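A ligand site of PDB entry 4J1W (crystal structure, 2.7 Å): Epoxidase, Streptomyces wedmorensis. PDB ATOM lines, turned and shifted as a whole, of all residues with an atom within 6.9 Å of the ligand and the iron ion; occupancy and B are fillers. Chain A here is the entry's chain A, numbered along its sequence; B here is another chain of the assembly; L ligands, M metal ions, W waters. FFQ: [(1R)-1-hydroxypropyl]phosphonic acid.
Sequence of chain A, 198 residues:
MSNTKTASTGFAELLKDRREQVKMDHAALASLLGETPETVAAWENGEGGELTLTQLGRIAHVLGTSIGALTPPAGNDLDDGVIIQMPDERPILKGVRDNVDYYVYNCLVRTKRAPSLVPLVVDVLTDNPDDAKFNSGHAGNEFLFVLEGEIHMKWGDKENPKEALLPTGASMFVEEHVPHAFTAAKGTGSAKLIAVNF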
ATOM      1  N   ARG A  97      -4.825 -25.143 -30.790  1.00  0.00           N
ATOM      2  CA  ARG A  97      -3.691 -24.491 -31.431  1.00  0.00           C
ATOM      3  C   ARG A  97      -2.768 -25.580 -31.971  1.00  0.00           C
ATOM      4  O   ARG A  97      -2.181 -26.347 -31.188  1.00  0.00           O
ATOM      5  CB  ARG A  97      -2.933 -23.605 -30.435  1.00  0.00           C
ATOM      6  CG  ARG A  97      -3.809 -22.518 -29.828  1.00  0.00           C
ATOM      7  CD  ARG A  97      -3.007 -21.471 -29.082  1.00  0.00           C
ATOM      8  NE  ARG A  97      -3.899 -20.479 -28.493  1.00  0.00           N
ATOM      9  CZ  ARG A  97      -3.501 -19.385 -27.850  1.00  0.00           C
ATOM     10  NH1 ARG A  97      -2.215 -19.119 -27.694  1.00  0.00           N
ATOM     11  NH2 ARG A  97      -4.412 -18.557 -27.355  1.00  0.00           N
ATOM     12  N   TYR A 103      -6.138 -25.089 -24.624  1.00  0.00           N
ATOM     13  CA  TYR A 103      -6.892 -24.506 -23.531  1.00  0.00           C
ATOM     14  C   TYR A 103      -8.327 -25.021 -23.507  1.00  0.00           C
ATOM     15  O   TYR A 103      -8.766 -25.702 -24.431  1.00  0.00           O
ATOM     16  CB  TYR A 103      -6.948 -22.990 -23.684  1.00  0.00           C
ATOM     17  CG  TYR A 103      -5.636 -22.245 -23.614  1.00  0.00           C
ATOM     18  CD1 TYR A 103      -5.464 -21.031 -24.315  1.00  0.00           C
ATOM     19  CD2 TYR A 103      -4.583 -22.689 -22.804  1.00  0.00           C
ATOM     20  CE1 TYR A 103      -4.296 -20.291 -24.207  1.00  0.00           C
ATOM     21  CE2 TYR A 103      -3.395 -21.946 -22.696  1.00  0.00           C
ATOM     22  CZ  TYR A 103      -3.261 -20.743 -23.407  1.00  0.00           C
ATOM     23  OH  TYR A 103      -2.103 -20.001 -23.314  1.00  0.00           O
ATOM     24  N   TYR A 105     -11.820 -23.043 -22.364  1.00  0.00           N
ATOM     25  CA  TYR A 105     -12.389 -21.809 -21.840  1.00  0.00           C
ATOM     26  C   TYR A 105     -13.746 -21.935 -21.178  1.00  0.00           C
ATOM     27  O   TYR A 105     -14.729 -22.298 -21.824  1.00  0.00           O
ATOM     28  CB  TYR A 105     -12.498 -20.760 -22.944  1.00  0.00           C
ATOM     29  CG  TYR A 105     -11.220 -20.431 -23.642  1.00  0.00           C
ATOM     30  CD1 TYR A 105     -10.831 -21.113 -24.795  1.00  0.00           C
ATOM     31  CD2 TYR A 105     -10.393 -19.411 -23.180  1.00  0.00           C
ATOM     32  CE1 TYR A 105      -9.688 -20.775 -25.474  1.00  0.00           C
ATOM     33  CE2 TYR A 105      -9.242 -19.058 -23.855  1.00  0.00           C
ATOM     34  CZ  TYR A 105      -8.894 -19.741 -25.002  1.00  0.00           C
ATOM     35  OH  TYR A 105      -7.765 -19.362 -25.707  1.00  0.00           O
ATOM     36  N   LEU A 120     -12.649 -15.262 -17.859  1.00  0.00           N
ATOM     37  CA  LEU A 120     -12.616 -16.687 -18.136  1.00  0.00           C
ATOM     38  C   LEU A 120     -11.864 -17.525 -17.110  1.00  0.00           C
ATOM     39  O   LEU A 120     -10.928 -17.051 -16.466  1.00  0.00           O
ATOM     40  CB  LEU A 120     -11.927 -16.922 -19.477  1.00  0.00           C
ATOM     41  CG  LEU A 120     -12.372 -16.092 -20.671  1.00  0.00           C
ATOM     42  CD1 LEU A 120     -11.216 -15.964 -21.646  1.00  0.00           C
ATOM     43  CD2 LEU A 120     -13.581 -16.761 -21.339  1.00  0.00           C
ATOM     44  N   VAL A 122      -9.606 -20.585 -17.275  1.00  0.00           N
ATOM     45  CA  VAL A 122      -8.970 -21.334 -18.350  1.00  0.00           C
ATOM     46  C   VAL A 122      -8.208 -22.571 -17.896  1.00  0.00           C
ATOM     47  O   VAL A 122      -7.286 -22.485 -17.076  1.00  0.00           O
ATOM     48  CB  VAL A 122      -7.976 -20.435 -19.121  1.00  0.00           C
ATOM     49  CG1 VAL A 122      -7.331 -21.213 -20.247  1.00  0.00           C
ATOM     50  CG2 VAL A 122      -8.711 -19.204 -19.649  1.00  0.00           C
ATOM     51  N   VAL A 124      -5.507 -25.064 -18.505  1.00  0.00           N
ATOM     52  CA  VAL A 124      -4.300 -25.148 -19.315  1.00  0.00           C
ATOM     53  C   VAL A 124      -3.959 -26.640 -19.387  1.00  0.00           C
ATOM     54  O   VAL A 124      -3.473 -27.227 -18.421  1.00  0.00           O
ATOM     55  CB  VAL A 124      -3.158 -24.359 -18.669  1.00  0.00           C
ATOM     56  CG1 VAL A 124      -1.933 -24.388 -19.565  1.00  0.00           C
ATOM     57  CG2 VAL A 124      -3.593 -22.935 -18.420  1.00  0.00           C
ATOM     58  N   LYS A 133       2.243 -22.435 -27.453  1.00  0.00           N
ATOM     59  CA  LYS A 133       1.644 -21.859 -28.653  1.00  0.00           C
ATOM     60  C   LYS A 133       1.205 -20.418 -28.392  1.00  0.00           C
ATOM     61  O   LYS A 133       0.281 -20.173 -27.619  1.00  0.00           O
ATOM     62  CB  LYS A 133       0.456 -22.721 -29.078  1.00  0.00           C
ATOM     63  CG  LYS A 133       0.829 -24.160 -29.420  1.00  0.00           C
ATOM     64  CD  LYS A 133       1.520 -24.256 -30.783  1.00  0.00           C
ATOM     65  CE  LYS A 133       2.111 -25.638 -31.031  1.00  0.00           C
ATOM     66  NZ  LYS A 133       3.315 -25.886 -30.194  1.00  0.00           N
ATOM     67  N   PHE A 134       1.880 -19.479 -29.038  1.00  0.00           N
ATOM     68  CA  PHE A 134       1.593 -18.050 -28.885  1.00  0.00           C
ATOM     69  C   PHE A 134       0.391 -17.520 -29.641  1.00  0.00           C
ATOM     70  O   PHE A 134       0.092 -17.967 -30.748  1.00  0.00           O
ATOM     71  CB  PHE A 134       2.789 -17.214 -29.366  1.00  0.00           C
ATOM     72  CG  PHE A 134       3.852 -17.016 -28.344  1.00  0.00           C
ATOM     73  CD1 PHE A 134       4.640 -18.079 -27.917  1.00  0.00           C
ATOM     74  CD2 PHE A 134       4.111 -15.748 -27.835  1.00  0.00           C
ATOM     75  CE1 PHE A 134       5.670 -17.880 -27.005  1.00  0.00           C
ATOM     76  CE2 PHE A 134       5.139 -15.540 -26.929  1.00  0.00           C
ATOM     77  CZ  PHE A 134       5.920 -16.610 -26.511  1.00  0.00           C
ATOM     78  N   ASN A 135      -0.293 -16.564 -29.033  1.00  0.00           N
ATOM     79  CA  ASN A 135      -1.391 -15.890 -29.704  1.00  0.00           C
ATOM     80  C   ASN A 135      -0.590 -14.694 -30.235  1.00  0.00           C
ATOM     81  O   ASN A 135       0.574 -14.528 -29.854  1.00  0.00           O
ATOM     82  CB  ASN A 135      -2.465 -15.421 -28.723  1.00  0.00           C
ATOM     83  CG  ASN A 135      -1.919 -14.521 -27.629  1.00  0.00           C
ATOM     84  OD1 ASN A 135      -1.068 -13.663 -27.874  1.00  0.00           O
ATOM     85  ND2 ASN A 135      -2.426 -14.695 -26.419  1.00  0.00           N
ATOM     86  N   SER A 136      -1.170 -13.871 -31.084  1.00  0.00           N
ATOM     87  CA  SER A 136      -0.430 -12.739 -31.634  1.00  0.00           C
ATOM     88  C   SER A 136      -0.710 -11.442 -30.879  1.00  0.00           C
ATOM     89  O   SER A 136      -0.619 -10.361 -31.456  1.00  0.00           O
ATOM     90  CB  SER A 136      -0.767 -12.558 -33.111  1.00  0.00           C
ATOM     91  OG  SER A 136      -2.171 -12.440 -33.286  1.00  0.00           O
ATOM     92  N   GLY A 137      -1.040 -11.544 -29.600  1.00  0.00           N
ATOM     93  CA  GLY A 137      -1.355 -10.360 -28.832  1.00  0.00           C
ATOM     94  C   GLY A 137      -2.759  -9.944 -29.215  1.00  0.00           C
ATOM     95  O   GLY A 137      -3.229 -10.267 -30.316  1.00  0.00           O
ATOM     96  N   HIS A 138      -3.465  -9.247 -28.331  1.00  0.00           N
ATOM     97  CA  HIS A 138      -4.815  -8.822 -28.629  1.00  0.00           C
ATOM     98  C   HIS A 138      -5.183  -7.496 -27.987  1.00  0.00           C
ATOM     99  O   HIS A 138      -4.518  -7.036 -27.062  1.00  0.00           O
ATOM    100  CB  HIS A 138      -5.828  -9.908 -28.208  1.00  0.00           C
ATOM    101  CG  HIS A 138      -5.669 -10.364 -26.786  1.00  0.00           C
ATOM    102  ND1 HIS A 138      -5.878  -9.565 -25.684  1.00  0.00           N
ATOM    103  CD2 HIS A 138      -5.310 -11.571 -26.286  1.00  0.00           C
ATOM    104  CE1 HIS A 138      -5.646 -10.288 -24.586  1.00  0.00           C
ATOM    105  NE2 HIS A 138      -5.294 -11.521 -24.912  1.00  0.00           N
ATOM    106  N   GLU A 142      -5.210  -7.436 -19.986  1.00  0.00           N
ATOM    107  CA  GLU A 142      -5.694  -8.673 -19.404  1.00  0.00           C
ATOM    108  C   GLU A 142      -5.085  -8.927 -18.040  1.00  0.00           C
ATOM    109  O   GLU A 142      -3.877  -8.759 -17.840  1.00  0.00           O
ATOM    110  CB  GLU A 142      -5.390  -9.837 -20.350  1.00  0.00           C
ATOM    111  CG  GLU A 142      -5.616 -11.224 -19.792  1.00  0.00           C
ATOM    112  CD  GLU A 142      -5.468 -12.301 -20.859  1.00  0.00           C
ATOM    113  OE1 GLU A 142      -4.783 -12.059 -21.870  1.00  0.00           O
ATOM    114  OE2 GLU A 142      -6.036 -13.398 -20.675  1.00  0.00           O
ATOM    115  N   LEU A 144      -4.524 -11.730 -15.018  1.00  0.00           N
ATOM    116  CA  LEU A 144      -4.474 -13.175 -14.803  1.00  0.00           C
ATOM    117  C   LEU A 144      -4.226 -13.501 -13.337  1.00  0.00           C
ATOM    118  O   LEU A 144      -3.602 -12.736 -12.619  1.00  0.00           O
ATOM    119  CB  LEU A 144      -3.336 -13.809 -15.619  1.00  0.00           C
ATOM    120  CG  LEU A 144      -3.271 -13.849 -17.149  1.00  0.00           C
ATOM    121  CD1 LEU A 144      -4.401 -14.702 -17.687  1.00  0.00           C
ATOM    122  CD2 LEU A 144      -3.329 -12.446 -17.727  1.00  0.00           C
ATOM    123  N   VAL A 174      -1.034  -8.208 -18.488  1.00  0.00           N
ATOM    124  CA  VAL A 174      -0.471  -8.216 -19.817  1.00  0.00           C
ATOM    125  C   VAL A 174      -1.114  -7.084 -20.588  1.00  0.00           C
ATOM    126  O   VAL A 174      -2.331  -7.106 -20.816  1.00  0.00           O
ATOM    127  CB  VAL A 174      -0.755  -9.549 -20.548  1.00  0.00           C
ATOM    128  CG1 VAL A 174      -0.236  -9.484 -21.985  1.00  0.00           C
ATOM    129  CG2 VAL A 174      -0.117 -10.705 -19.800  1.00  0.00           C
ATOM    130  N   VAL A 178       0.424  -7.332 -26.512  1.00  0.00           N
ATOM    131  CA  VAL A 178       1.621  -8.061 -26.108  1.00  0.00           C
ATOM    132  C   VAL A 178       1.314  -9.550 -26.332  1.00  0.00           C
ATOM    133  O   VAL A 178       0.400 -10.096 -25.730  1.00  0.00           O
ATOM    134  CB  VAL A 178       1.960  -7.861 -24.618  1.00  0.00           C
ATOM    135  CG1 VAL A 178       3.182  -8.683 -24.238  1.00  0.00           C
ATOM    136  CG2 VAL A 178       2.183  -6.388 -24.328  1.00  0.00           C
ATOM    137  N   HIS A 180       1.435 -13.448 -25.908  1.00  0.00           N
ATOM    138  CA  HIS A 180       1.722 -14.289 -24.745  1.00  0.00           C
ATOM    139  C   HIS A 180       1.307 -15.735 -24.976  1.00  0.00           C
ATOM    140  O   HIS A 180       0.568 -16.038 -25.898  1.00  0.00           O
ATOM    141  CB  HIS A 180       1.001 -13.731 -23.503  1.00  0.00           C
ATOM    142  CG  HIS A 180      -0.399 -13.262 -23.776  1.00  0.00           C
ATOM    143  ND1 HIS A 180      -0.694 -12.111 -24.479  1.00  0.00           N
ATOM    144  CD2 HIS A 180      -1.594 -13.816 -23.470  1.00  0.00           C
ATOM    145  CE1 HIS A 180      -2.030 -12.005 -24.590  1.00  0.00           C
ATOM    146  NE2 HIS A 180      -2.620 -13.021 -23.990  1.00  0.00           N
ATOM    147  N   ALA A 181       1.794 -16.624 -24.103  1.00  0.00           N
ATOM    148  CA  ALA A 181       1.466 -18.033 -24.190  1.00  0.00           C
ATOM    149  C   ALA A 181       1.641 -18.700 -22.830  1.00  0.00           C
ATOM    150  O   ALA A 181       2.528 -18.296 -22.060  1.00  0.00           O
ATOM    151  CB  ALA A 181       2.363 -18.721 -25.211  1.00  0.00           C
ATOM    152  N   PHE A 182       0.806 -19.692 -22.540  1.00  0.00           N
ATOM    153  CA  PHE A 182       0.893 -20.405 -21.261  1.00  0.00           C
ATOM    154  C   PHE A 182       0.819 -21.919 -21.433  1.00  0.00           C
ATOM    155  O   PHE A 182       0.244 -22.423 -22.388  1.00  0.00           O
ATOM    156  CB  PHE A 182      -0.274 -20.034 -20.331  1.00  0.00           C
ATOM    157  CG  PHE A 182      -0.478 -18.572 -20.138  1.00  0.00           C
ATOM    158  CD1 PHE A 182      -1.367 -17.870 -20.955  1.00  0.00           C
ATOM    159  CD2 PHE A 182       0.219 -17.889 -19.139  1.00  0.00           C
ATOM    160  CE1 PHE A 182      -1.557 -16.501 -20.764  1.00  0.00           C
ATOM    161  CE2 PHE A 182       0.039 -16.523 -18.934  1.00  0.00           C
ATOM    162  CZ  PHE A 182      -0.849 -15.825 -19.760  1.00  0.00           C
ATOM    163  N   LEU A 193      -6.120 -21.175 -14.604  1.00  0.00           N
ATOM    164  CA  LEU A 193      -6.034 -19.780 -14.221  1.00  0.00           C
ATOM    165  C   LEU A 193      -7.275 -18.972 -14.583  1.00  0.00           C
ATOM    166  O   LEU A 193      -8.097 -19.408 -15.360  1.00  0.00           O
ATOM    167  CB  LEU A 193      -4.785 -19.155 -14.850  1.00  0.00           C
ATOM    168  CG  LEU A 193      -4.657 -19.153 -16.360  1.00  0.00           C
ATOM    169  CD1 LEU A 193      -5.622 -18.130 -16.920  1.00  0.00           C
ATOM    170  CD2 LEU A 193      -3.230 -18.808 -16.764  1.00  0.00           C
ATOM    171  N   ILE A 194      -7.405 -17.807 -13.961  1.00  0.00           N
ATOM    172  CA  ILE A 194      -8.535 -16.909 -14.230  1.00  0.00           C
ATOM    173  C   ILE A 194      -7.970 -15.808 -15.094  1.00  0.00           C
ATOM    174  O   ILE A 194      -6.946 -15.210 -14.787  1.00  0.00           O
ATOM    175  CB  ILE A 194      -9.098 -16.278 -12.935  1.00  0.00           C
ATOM    176  CG1 ILE A 194      -9.696 -17.377 -12.043  1.00  0.00           C
ATOM    177  CG2 ILE A 194     -10.168 -15.268 -13.283  1.00  0.00           C
ATOM    178  CD1 ILE A 194     -10.400 -16.855 -10.825  1.00  0.00           C
ATOM    179  N   ALA A 195      -8.637 -15.553 -16.211  1.00  0.00           N
ATOM    180  CA  ALA A 195      -8.180 -14.516 -17.124  1.00  0.00           C
ATOM    181  C   ALA A 195      -9.292 -13.513 -17.300  1.00  0.00           C
ATOM    182  O   ALA A 195     -10.397 -13.862 -17.705  1.00  0.00           O
ATOM    183  CB  ALA A 195      -7.809 -15.132 -18.458  1.00  0.00           C
ATOM    184  N   ASN A 197     -10.211 -10.166 -19.305  1.00  0.00           N
ATOM    185  CA  ASN A 197      -9.910  -9.175 -20.345  1.00  0.00           C
ATOM    186  C   ASN A 197     -10.860  -8.036 -20.107  1.00  0.00           C
ATOM    187  O   ASN A 197     -12.049  -8.248 -19.894  1.00  0.00           O
ATOM    188  CB  ASN A 197     -10.147  -9.770 -21.730  1.00  0.00           C
ATOM    189  CG  ASN A 197      -9.351 -11.031 -21.969  1.00  0.00           C
ATOM    190  OD1 ASN A 197      -8.176 -10.979 -22.348  1.00  0.00           O
ATOM    191  ND2 ASN A 197      -9.987 -12.179 -21.719  1.00  0.00           N
ATOM    192  N   GLU B  20     -14.071 -14.117 -31.632  1.00  0.00           N
ATOM    193  CA  GLU B  20     -12.899 -14.665 -30.999  1.00  0.00           C
ATOM    194  C   GLU B  20     -12.681 -14.165 -29.574  1.00  0.00           C
ATOM    195  O   GLU B  20     -12.244 -14.917 -28.718  1.00  0.00           O
ATOM    196  CB  GLU B  20     -11.648 -14.359 -31.829  1.00  0.00           C
ATOM    197  CG  GLU B  20     -11.636 -15.081 -33.159  1.00  0.00           C
ATOM    198  CD  GLU B  20     -10.368 -14.838 -33.961  1.00  0.00           C
ATOM    199  OE1 GLU B  20     -10.194 -15.494 -35.012  1.00  0.00           O
ATOM    200  OE2 GLU B  20      -9.544 -13.985 -33.542  1.00  0.00           O
ATOM    201  N   LYS B  23     -14.681 -16.107 -27.156  1.00  0.00           N
ATOM    202  CA  LYS B  23     -14.336 -17.506 -27.329  1.00  0.00           C
ATOM    203  C   LYS B  23     -15.267 -18.425 -28.111  1.00  0.00           C
ATOM    204  O   LYS B  23     -15.140 -19.649 -28.011  1.00  0.00           O
ATOM    205  CB  LYS B  23     -14.078 -18.124 -25.961  1.00  0.00           C
ATOM    206  CG  LYS B  23     -13.067 -17.349 -25.140  1.00  0.00           C
ATOM    207  CD  LYS B  23     -11.801 -17.093 -25.939  1.00  0.00           C
ATOM    208  CE  LYS B  23     -10.870 -16.180 -25.165  1.00  0.00           C
ATOM    209  NZ  LYS B  23      -9.663 -15.816 -25.930  1.00  0.00           N
HETATM  210  C1  FFQ L   1      -5.812 -17.157 -22.112  1.00  0.00           C
HETATM  211  O1  FFQ L   1      -4.728 -15.023 -22.476  1.00  0.00           O
HETATM  212  P1  FFQ L   1      -5.762 -16.030 -24.741  1.00  0.00           P
HETATM  213  C2  FFQ L   1      -4.983 -16.286 -23.057  1.00  0.00           C
HETATM  214  O2  FFQ L   1      -7.006 -16.856 -24.880  1.00  0.00           O
HETATM  215  C3  FFQ L   1      -5.149 -17.366 -20.741  1.00  0.00           C
HETATM  216  O3  FFQ L   1      -6.127 -14.458 -24.941  1.00  0.00           O
HETATM  217  O4  FFQ L   1      -4.688 -16.437 -25.851  1.00  0.00           O
HETATM  218 FE    FE M   1      -4.850 -13.293 -23.709  1.00  0.00          FE
HETATM  219  O   HOH W   1      -1.755 -17.614 -25.121  1.00  0.00           O
HETATM  220  O   HOH W   2      -8.141 -14.303 -22.633  1.00  0.00           O
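Water W2 lies within hydrogen-bond range of ND2 of Asn 197 and OE2 of Glu 142.
Water W1 lies within hydrogen-bond range of O of His 180 (2.9 Å), OH of Tyr 103 (3.0 Å), NH1 of Arg 97 (3.0 Å), O4 of the ligand (3.2 Å) and ND2 of Asn 135 (3.3 Å).
The iron ion is bound by an oxygen (O3) of the ligand, an oxygen (O1) of the ligand, a ring nitrogen (NE2) of His 138, the side-chain carboxylate of Glu 142 and a ring nitrogen (NE2) of His 180.
The iron ion has five donor atoms within binding distance.
Asn 135 touches the iron ion (ND2 to FE, 3.9 Å).
Phe 182 touches the ligand (CE1 to C3, 3.7 Å).
Leu 193 touches the ligand (CD1 to C3, 3.9 Å).
Hydrophobic or aromatic side chains within 4 Å of the ligand: Tyr 105, His 138, His 180, Phe 182 and Leu 193.
Along chain A the residues within 4 Å of the ligand span positions 97 to 193.
The nearest printed residue that does not touch the ligand is Tyr 103 (4.1 Å).
OH of Tyr 105 lies within hydrogen-bond range of O2 of the ligand.
The side-chain amide nitrogen (ND2) of Asn 135 is in hydrogen-bond range of an oxygen (O4) of the ligand.
O2 of the ligand is in salt-bridge range of NZ of Lys 23 of chain B (3.0 Å).
O4 of the ligand lies within salt-bridge range of NH2 of Arg 97.
OH of Tyr 103 sits at hydrogen-bond distance from N of Phe 182 (3.0 Å).
N of Val 122 lies within hydrogen-bond range of O of Leu 193 (2.7 Å).
The side-chain amide oxygen (OD1) of Asn 135 sits at hydrogen-bond distance from the backbone NH (N) of Gly 137, at 2.7 Å.
The side-chain amide oxygen of Asn 135 sits at hydrogen-bond distance from the backbone NH of His 180.
O of Glu 142 lies within hydrogen-bond range of N of Val 174 (3.0 Å).
ND1 of His 180 is in hydrogen-bond range of O of Val 178, 2.6 Å away.
NH1 of Arg 97 is in hydrogen-bond range of O of Lys 133 (2.7 Å).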
